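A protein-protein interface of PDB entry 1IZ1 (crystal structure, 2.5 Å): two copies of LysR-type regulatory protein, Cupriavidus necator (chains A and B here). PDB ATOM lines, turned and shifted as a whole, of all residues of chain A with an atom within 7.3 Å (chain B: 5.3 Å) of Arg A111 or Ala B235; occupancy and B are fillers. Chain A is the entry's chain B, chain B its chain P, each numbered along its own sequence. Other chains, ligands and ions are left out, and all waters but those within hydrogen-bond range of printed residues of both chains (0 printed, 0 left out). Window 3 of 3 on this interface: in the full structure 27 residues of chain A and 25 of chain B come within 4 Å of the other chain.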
ATOM      1  N   ARG A 104      29.457 -31.402  19.545  1.00  0.00           N
ATOM      2  CA  ARG A 104      28.989 -30.045  19.824  1.00  0.00           C
ATOM      3  C   ARG A 104      29.752 -28.951  19.093  1.00  0.00           C
ATOM      4  O   ARG A 104      29.168 -28.191  18.351  1.00  0.00           O
ATOM      5  CB  ARG A 104      29.029 -29.758  21.347  1.00  0.00           C
ATOM      6  CG  ARG A 104      28.302 -28.475  21.790  1.00  0.00           C
ATOM      7  CD  ARG A 104      26.805 -28.407  21.358  1.00  0.00           C
ATOM      8  NE  ARG A 104      26.119 -27.166  21.746  1.00  0.00           N
ATOM      9  CZ  ARG A 104      24.934 -26.786  21.267  1.00  0.00           C
ATOM     10  NH1 ARG A 104      24.298 -27.547  20.377  1.00  0.00           N
ATOM     11  NH2 ARG A 104      24.369 -25.652  21.674  1.00  0.00           N
ATOM     12  N   SER A 105      31.055 -28.880  19.300  1.00  0.00           N
ATOM     13  CA  SER A 105      31.839 -27.756  18.803  1.00  0.00           C
ATOM     14  C   SER A 105      31.811 -27.653  17.293  1.00  0.00           C
ATOM     15  O   SER A 105      31.746 -26.557  16.756  1.00  0.00           O
ATOM     16  CB  SER A 105      33.292 -27.822  19.327  1.00  0.00           C
ATOM     17  OG  SER A 105      33.628 -29.122  19.802  1.00  0.00           O
ATOM     18  N   LEU A 106      31.877 -28.783  16.596  1.00  0.00           N
ATOM     19  CA  LEU A 106      31.837 -28.783  15.128  1.00  0.00           C
ATOM     20  C   LEU A 106      30.476 -28.434  14.538  1.00  0.00           C
ATOM     21  O   LEU A 106      30.416 -27.669  13.572  1.00  0.00           O
ATOM     22  CB  LEU A 106      32.305 -30.117  14.555  1.00  0.00           C
ATOM     23  CG  LEU A 106      32.274 -30.282  13.039  1.00  0.00           C
ATOM     24  CD1 LEU A 106      32.966 -29.089  12.370  1.00  0.00           C
ATOM     25  CD2 LEU A 106      32.958 -31.592  12.688  1.00  0.00           C
ATOM     26  N   PRO A 107      29.399 -29.031  15.048  1.00  0.00           N
ATOM     27  CA  PRO A 107      28.053 -28.579  14.693  1.00  0.00           C
ATOM     28  C   PRO A 107      27.850 -27.053  14.793  1.00  0.00           C
ATOM     29  O   PRO A 107      27.312 -26.484  13.862  1.00  0.00           O
ATOM     30  CB  PRO A 107      27.164 -29.330  15.684  1.00  0.00           C
ATOM     31  CG  PRO A 107      27.894 -30.553  15.995  1.00  0.00           C
ATOM     32  CD  PRO A 107      29.355 -30.231  15.891  1.00  0.00           C
ATOM     33  N   LEU A 108      28.300 -26.404  15.856  1.00  0.00           N
ATOM     34  CA  LEU A 108      28.070 -24.963  16.000  1.00  0.00           C
ATOM     35  C   LEU A 108      28.826 -24.157  14.954  1.00  0.00           C
ATOM     36  O   LEU A 108      28.292 -23.197  14.365  1.00  0.00           O
ATOM     37  CB  LEU A 108      28.487 -24.464  17.378  1.00  0.00           C
ATOM     38  CG  LEU A 108      27.590 -24.874  18.533  1.00  0.00           C
ATOM     39  CD1 LEU A 108      28.116 -24.211  19.817  1.00  0.00           C
ATOM     40  CD2 LEU A 108      26.093 -24.540  18.287  1.00  0.00           C
ATOM     41  N   LEU A 109      30.080 -24.544  14.747  1.00  0.00           N
ATOM     42  CA  LEU A 109      30.897 -23.960  13.704  1.00  0.00           C
ATOM     43  C   LEU A 109      30.191 -24.020  12.385  1.00  0.00           C
ATOM     44  O   LEU A 109      30.169 -23.051  11.674  1.00  0.00           O
ATOM     45  CB  LEU A 109      32.221 -24.705  13.581  1.00  0.00           C
ATOM     46  CG  LEU A 109      33.482 -23.865  13.647  1.00  0.00           C
ATOM     47  CD1 LEU A 109      34.624 -24.733  13.143  1.00  0.00           C
ATOM     48  CD2 LEU A 109      33.370 -22.602  12.841  1.00  0.00           C
ATOM     49  N   LEU A 110      29.622 -25.171  12.049  1.00  0.00           N
ATOM     50  CA  LEU A 110      28.980 -25.359  10.751  1.00  0.00           C
ATOM     51  C   LEU A 110      27.711 -24.545  10.676  1.00  0.00           C
ATOM     52  O   LEU A 110      27.352 -24.081   9.623  1.00  0.00           O
ATOM     53  CB  LEU A 110      28.614 -26.824  10.530  1.00  0.00           C
ATOM     54  CG  LEU A 110      29.736 -27.856  10.411  1.00  0.00           C
ATOM     55  CD1 LEU A 110      29.170 -29.227  10.036  1.00  0.00           C
ATOM     56  CD2 LEU A 110      30.787 -27.386   9.410  1.00  0.00           C
ATOM     57  N   ARG A 111      27.029 -24.381  11.798  1.00  0.00           N
ATOM     58  CA  ARG A 111      25.765 -23.675  11.811  1.00  0.00           C
ATOM     59  C   ARG A 111      25.999 -22.229  11.455  1.00  0.00           C
ATOM     60  O   ARG A 111      25.229 -21.644  10.725  1.00  0.00           O
ATOM     61  CB  ARG A 111      25.079 -23.802  13.174  1.00  0.00           C
ATOM     62  CG  ARG A 111      23.725 -23.130  13.266  1.00  0.00           C
ATOM     63  CD  ARG A 111      23.018 -23.364  14.616  1.00  0.00           C
ATOM     64  NE  ARG A 111      22.473 -22.125  15.187  1.00  0.00           N
ATOM     65  CZ  ARG A 111      23.206 -21.087  15.630  1.00  0.00           C
ATOM     66  NH1 ARG A 111      24.538 -21.116  15.585  1.00  0.00           N
ATOM     67  NH2 ARG A 111      22.600 -20.006  16.127  1.00  0.00           N
ATOM     68  N   ALA A 112      27.069 -21.656  11.958  1.00  0.00           N
ATOM     69  CA  ALA A 112      27.421 -20.289  11.615  1.00  0.00           C
ATOM     70  C   ALA A 112      27.769 -20.186  10.137  1.00  0.00           C
ATOM     71  O   ALA A 112      27.346 -19.249   9.459  1.00  0.00           O
ATOM     72  CB  ALA A 112      28.579 -19.841  12.441  1.00  0.00           C
ATOM     73  N   PHE A 113      28.529 -21.156   9.634  1.00  0.00           N
ATOM     74  CA  PHE A 113      28.974 -21.123   8.251  1.00  0.00           C
ATOM     75  C   PHE A 113      27.789 -21.193   7.322  1.00  0.00           C
ATOM     76  O   PHE A 113      27.702 -20.415   6.395  1.00  0.00           O
ATOM     77  CB  PHE A 113      29.971 -22.245   7.943  1.00  0.00           C
ATOM     78  CG  PHE A 113      30.197 -22.476   6.473  1.00  0.00           C
ATOM     79  CD1 PHE A 113      30.888 -21.552   5.704  1.00  0.00           C
ATOM     80  CD2 PHE A 113      29.718 -23.613   5.851  1.00  0.00           C
ATOM     81  CE1 PHE A 113      31.102 -21.771   4.342  1.00  0.00           C
ATOM     82  CE2 PHE A 113      29.922 -23.829   4.485  1.00  0.00           C
ATOM     83  CZ  PHE A 113      30.612 -22.908   3.735  1.00  0.00           C
ATOM     84  N   LEU A 114      26.865 -22.101   7.593  1.00  0.00           N
ATOM     85  CA  LEU A 114      25.754 -22.402   6.687  1.00  0.00           C
ATOM     86  C   LEU A 114      24.709 -21.327   6.744  1.00  0.00           C
ATOM     87  O   LEU A 114      24.044 -21.042   5.759  1.00  0.00           O
ATOM     88  CB  LEU A 114      25.107 -23.743   7.042  1.00  0.00           C
ATOM     89  CG  LEU A 114      25.822 -24.949   6.425  1.00  0.00           C
ATOM     90  CD1 LEU A 114      25.240 -26.238   6.993  1.00  0.00           C
ATOM     91  CD2 LEU A 114      25.723 -24.938   4.903  1.00  0.00           C
ATOM     92  N   THR A 115      24.571 -20.741   7.919  1.00  0.00           N
ATOM     93  CA  THR A 115      23.768 -19.548   8.111  1.00  0.00           C
ATOM     94  C   THR A 115      24.297 -18.331   7.324  1.00  0.00           C
ATOM     95  O   THR A 115      23.504 -17.531   6.809  1.00  0.00           O
ATOM     96  CB  THR A 115      23.703 -19.253   9.641  1.00  0.00           C
ATOM     97  OG1 THR A 115      22.990 -20.307  10.300  1.00  0.00           O
ATOM     98  CG2 THR A 115      22.892 -18.020   9.936  1.00  0.00           C
ATOM     99  N   SER A 116      25.619 -18.183   7.239  1.00  0.00           N
ATOM    100  CA  SER A 116      26.230 -17.028   6.557  1.00  0.00           C
ATOM    101  C   SER A 116      26.365 -17.254   5.062  1.00  0.00           C
ATOM    102  O   SER A 116      26.662 -16.313   4.313  1.00  0.00           O
ATOM    103  CB  SER A 116      27.617 -16.690   7.133  1.00  0.00           C
ATOM    104  OG  SER A 116      27.598 -16.746   8.553  1.00  0.00           O
ATOM    105  N   THR A 117      26.151 -18.502   4.640  1.00  0.00           N
ATOM    106  CA  THR A 117      26.295 -18.908   3.253  1.00  0.00           C
ATOM    107  C   THR A 117      25.158 -19.860   2.925  1.00  0.00           C
ATOM    108  O   THR A 117      25.387 -21.059   2.685  1.00  0.00           O
ATOM    109  CB  THR A 117      27.658 -19.608   3.018  1.00  0.00           C
ATOM    110  OG1 THR A 117      28.695 -18.987   3.795  1.00  0.00           O
ATOM    111  CG2 THR A 117      28.099 -19.463   1.546  1.00  0.00           C
ATOM    112  N   LEU A 124      29.338 -34.759   5.710  1.00  0.00           N
ATOM    113  CA  LEU A 124      30.148 -35.135   6.847  1.00  0.00           C
ATOM    114  C   LEU A 124      30.645 -36.573   6.708  1.00  0.00           C
ATOM    115  O   LEU A 124      29.910 -37.455   6.274  1.00  0.00           O
ATOM    116  CB  LEU A 124      29.320 -34.988   8.120  1.00  0.00           C
ATOM    117  CG  LEU A 124      29.362 -33.591   8.723  1.00  0.00           C
ATOM    118  CD1 LEU A 124      28.084 -33.297   9.528  1.00  0.00           C
ATOM    119  CD2 LEU A 124      30.606 -33.461   9.604  1.00  0.00           C
ATOM    120  N   PHE A 284      34.860 -20.878   4.446  1.00  0.00           N
ATOM    121  CA  PHE A 284      34.828 -21.598   5.721  1.00  0.00           C
ATOM    122  C   PHE A 284      36.026 -21.265   6.586  1.00  0.00           C
ATOM    123  O   PHE A 284      35.916 -21.290   7.792  1.00  0.00           O
ATOM    124  CB  PHE A 284      34.797 -23.102   5.520  1.00  0.00           C
ATOM    125  CG  PHE A 284      34.603 -23.866   6.796  1.00  0.00           C
ATOM    126  CD1 PHE A 284      33.459 -23.663   7.560  1.00  0.00           C
ATOM    127  CD2 PHE A 284      35.556 -24.787   7.238  1.00  0.00           C
ATOM    128  CE1 PHE A 284      33.251 -24.361   8.711  1.00  0.00           C
ATOM    129  CE2 PHE A 284      35.353 -25.480   8.404  1.00  0.00           C
ATOM    130  CZ  PHE A 284      34.189 -25.263   9.144  1.00  0.00           C
ATOM    131  N   HIS A 287      35.562 -18.110   8.407  1.00  0.00           N
ATOM    132  CA  HIS A 287      34.769 -18.362   9.602  1.00  0.00           C
ATOM    133  C   HIS A 287      35.518 -19.130  10.708  1.00  0.00           C
ATOM    134  O   HIS A 287      35.249 -18.972  11.910  1.00  0.00           O
ATOM    135  CB  HIS A 287      33.418 -19.027   9.326  1.00  0.00           C
ATOM    136  CG  HIS A 287      32.500 -18.878  10.494  1.00  0.00           C
ATOM    137  ND1 HIS A 287      31.916 -17.669  10.824  1.00  0.00           N
ATOM    138  CD2 HIS A 287      32.211 -19.725  11.512  1.00  0.00           C
ATOM    139  CE1 HIS A 287      31.252 -17.796  11.961  1.00  0.00           C
ATOM    140  NE2 HIS A 287      31.416 -19.034  12.400  1.00  0.00           N
ATOM    141  N   HIS B 170      15.678 -29.394  14.350  1.00  0.00           N
ATOM    142  CA  HIS B 170      16.393 -28.347  15.069  1.00  0.00           C
ATOM    143  C   HIS B 170      15.419 -27.692  16.062  1.00  0.00           C
ATOM    144  O   HIS B 170      14.220 -27.682  15.809  1.00  0.00           O
ATOM    145  CB  HIS B 170      16.939 -27.305  14.119  1.00  0.00           C
ATOM    146  CG  HIS B 170      17.756 -26.250  14.798  1.00  0.00           C
ATOM    147  ND1 HIS B 170      17.309 -24.956  14.965  1.00  0.00           N
ATOM    148  CD2 HIS B 170      18.982 -26.301  15.366  1.00  0.00           C
ATOM    149  CE1 HIS B 170      18.230 -24.258  15.601  1.00  0.00           C
ATOM    150  NE2 HIS B 170      19.261 -25.044  15.837  1.00  0.00           N
ATOM    151  N   ARG B 171      15.925 -27.163  17.181  1.00  0.00           N
ATOM    152  CA  ARG B 171      15.073 -26.622  18.280  1.00  0.00           C
ATOM    153  C   ARG B 171      14.140 -25.480  17.860  1.00  0.00           C
ATOM    154  O   ARG B 171      13.111 -25.253  18.494  1.00  0.00           O
ATOM    155  CB  ARG B 171      15.923 -26.169  19.492  1.00  0.00           C
ATOM    156  CG  ARG B 171      16.909 -25.066  19.212  1.00  0.00           C
ATOM    157  CD  ARG B 171      16.436 -23.658  19.612  1.00  0.00           C
ATOM    158  NE  ARG B 171      17.426 -23.047  20.508  1.00  0.00           N
ATOM    159  CZ  ARG B 171      18.570 -22.482  20.123  1.00  0.00           C
ATOM    160  NH1 ARG B 171      18.910 -22.404  18.842  1.00  0.00           N
ATOM    161  NH2 ARG B 171      19.384 -21.984  21.046  1.00  0.00           N
ATOM    162  N   LEU B 230      22.362 -36.381  13.161  1.00  0.00           N
ATOM    163  CA  LEU B 230      22.118 -35.679  14.437  1.00  0.00           C
ATOM    164  C   LEU B 230      22.881 -34.378  14.454  1.00  0.00           C
ATOM    165  O   LEU B 230      22.343 -33.376  14.883  1.00  0.00           O
ATOM    166  CB  LEU B 230      22.540 -36.522  15.626  1.00  0.00           C
ATOM    167  CG  LEU B 230      21.587 -37.682  15.933  1.00  0.00           C
ATOM    168  CD1 LEU B 230      22.092 -38.482  17.111  1.00  0.00           C
ATOM    169  CD2 LEU B 230      20.155 -37.194  16.207  1.00  0.00           C
ATOM    170  N   ALA B 231      24.110 -34.399  13.929  1.00  0.00           N
ATOM    171  CA  ALA B 231      24.968 -33.214  13.842  1.00  0.00           C
ATOM    172  C   ALA B 231      24.429 -32.184  12.881  1.00  0.00           C
ATOM    173  O   ALA B 231      24.475 -30.997  13.163  1.00  0.00           O
ATOM    174  CB  ALA B 231      26.389 -33.606  13.420  1.00  0.00           C
ATOM    175  N   LEU B 232      23.939 -32.628  11.738  1.00  0.00           N
ATOM    176  CA  LEU B 232      23.346 -31.733  10.782  1.00  0.00           C
ATOM    177  C   LEU B 232      22.056 -31.168  11.350  1.00  0.00           C
ATOM    178  O   LEU B 232      21.749 -30.017  11.143  1.00  0.00           O
ATOM    179  CB  LEU B 232      23.074 -32.468   9.485  1.00  0.00           C
ATOM    180  CG  LEU B 232      24.289 -32.904   8.662  1.00  0.00           C
ATOM    181  CD1 LEU B 232      23.865 -33.817   7.539  1.00  0.00           C
ATOM    182  CD2 LEU B 232      25.014 -31.701   8.117  1.00  0.00           C
ATOM    183  N   THR B 233      21.305 -31.974  12.082  1.00  0.00           N
ATOM    184  CA  THR B 233      20.104 -31.507  12.740  1.00  0.00           C
ATOM    185  C   THR B 233      20.444 -30.456  13.803  1.00  0.00           C
ATOM    186  O   THR B 233      19.776 -29.436  13.914  1.00  0.00           O
ATOM    187  CB  THR B 233      19.342 -32.684  13.383  1.00  0.00           C
ATOM    188  OG1 THR B 233      18.998 -33.650  12.383  1.00  0.00           O
ATOM    189  CG2 THR B 233      17.957 -32.227  13.942  1.00  0.00           C
ATOM    190  N   MET B 234      21.505 -30.713  14.554  1.00  0.00           N
ATOM    191  CA  MET B 234      21.944 -29.817  15.594  1.00  0.00           C
ATOM    192  C   MET B 234      22.374 -28.486  14.985  1.00  0.00           C
ATOM    193  O   MET B 234      22.175 -27.448  15.581  1.00  0.00           O
ATOM    194  CB  MET B 234      23.099 -30.461  16.380  1.00  0.00           C
ATOM    195  CG  MET B 234      23.581 -29.637  17.577  1.00  0.00           C
ATOM    196  SD  MET B 234      24.976 -30.375  18.357  1.00  0.00           S
ATOM    197  CE  MET B 234      24.263 -31.606  19.452  1.00  0.00           C
ATOM    198  N   ALA B 235      22.951 -28.531  13.795  1.00  0.00           N
ATOM    199  CA  ALA B 235      23.440 -27.331  13.126  1.00  0.00           C
ATOM    200  C   ALA B 235      22.364 -26.604  12.327  1.00  0.00           C
ATOM    201  O   ALA B 235      22.676 -25.723  11.537  1.00  0.00           O
ATOM    202  CB  ALA B 235      24.567 -27.709  12.190  1.00  0.00           C
ATOM    203  N   GLY B 236      21.109 -27.001  12.461  1.00  0.00           N
ATOM    204  CA  GLY B 236      20.041 -26.368  11.715  1.00  0.00           C
ATOM    205  C   GLY B 236      19.959 -26.682  10.237  1.00  0.00           C
ATOM    206  O   GLY B 236      19.252 -26.003   9.510  1.00  0.00           O
ATOM    207  N   ALA B 237      20.625 -27.725   9.782  1.00  0.00           N
ATOM    208  CA  ALA B 237      20.596 -28.047   8.360  1.00  0.00           C
ATOM    209  C   ALA B 237      19.838 -29.338   8.012  1.00  0.00           C
ATOM    210  O   ALA B 237      19.985 -29.837   6.901  1.00  0.00           O
ATOM    211  CB  ALA B 237      22.008 -28.116   7.843  1.00  0.00           C
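Among the printed residues, merely in contact across the chains: Arg A111 with Ala B235, Pro A107 with Ala B235, Pro A107 with Met B234, Leu A124 with Leu B232 and Leu A114 with Ala B237.
Of the printed residues of chain B, Arg A104 touches Met B234 (3.5 Å). Printed residues of chain B within 4 Å of Pro A107: Met B234 and Ala B235. Arg A111 touches one residue of chain B. Ser A116 touches none of the printed residues of chain B. Of the printed residues of chain B, Leu A124 touches Leu B232 (3.7 Å). Phe A284 touches none of the printed residues of chain B. Of the printed residues of chain A, Leu B232 touches Leu A124 (3.7 Å). Of chain A, only Pro A107 and Arg A111 come within 4 Å of Ala B235. Of the printed residues of chain A, Ala B237 touches Leu A114 (3.8 Å). The nearest residue of chain A that does not touch Ala B235 is Leu A110 (4.5 Å). The nearest printed residue of chain A that does not touch Ala B237 is Arg A111 (6.5 Å).
The guanidinium group of Arg A104 is in hydrogen-bond range of the side-chain sulfur of Met B234 (3.5 Å).
No position is printed for both chains. Of the 6 pairs that touch across the chains among the printed residues, none has its exchanged pair printed and touching as well.
Of the 17 printed residues of chain A, 5 touch a printed residue of chain B. Printed residues of chain A that touch a printed residue of chain B: Arg A104, Pro A107, Arg A111, Leu A114 and Leu A124. Hydrophobic or aromatic side chains of chain A that line the printed part of chain B: Pro A107, Leu A114 and Leu A124. Printed residues of chain B that touch a printed residue of chain A: Leu B232, Met B234, Ala B235 and Ala B237. Among the printed residues, 6 pairs touch across the chains. Among the printed residues, no Asp or Glu carboxylate lies within 4 Å of a Lys or Arg side-chain nitrogen of the other chain.
O of Arg A111 sits at hydrogen-bond distance from OG1 of Thr A115, at 2.6 Å. O of Leu B232 lies within hydrogen-bond range of N of Ala B237, at 2.9 Å.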
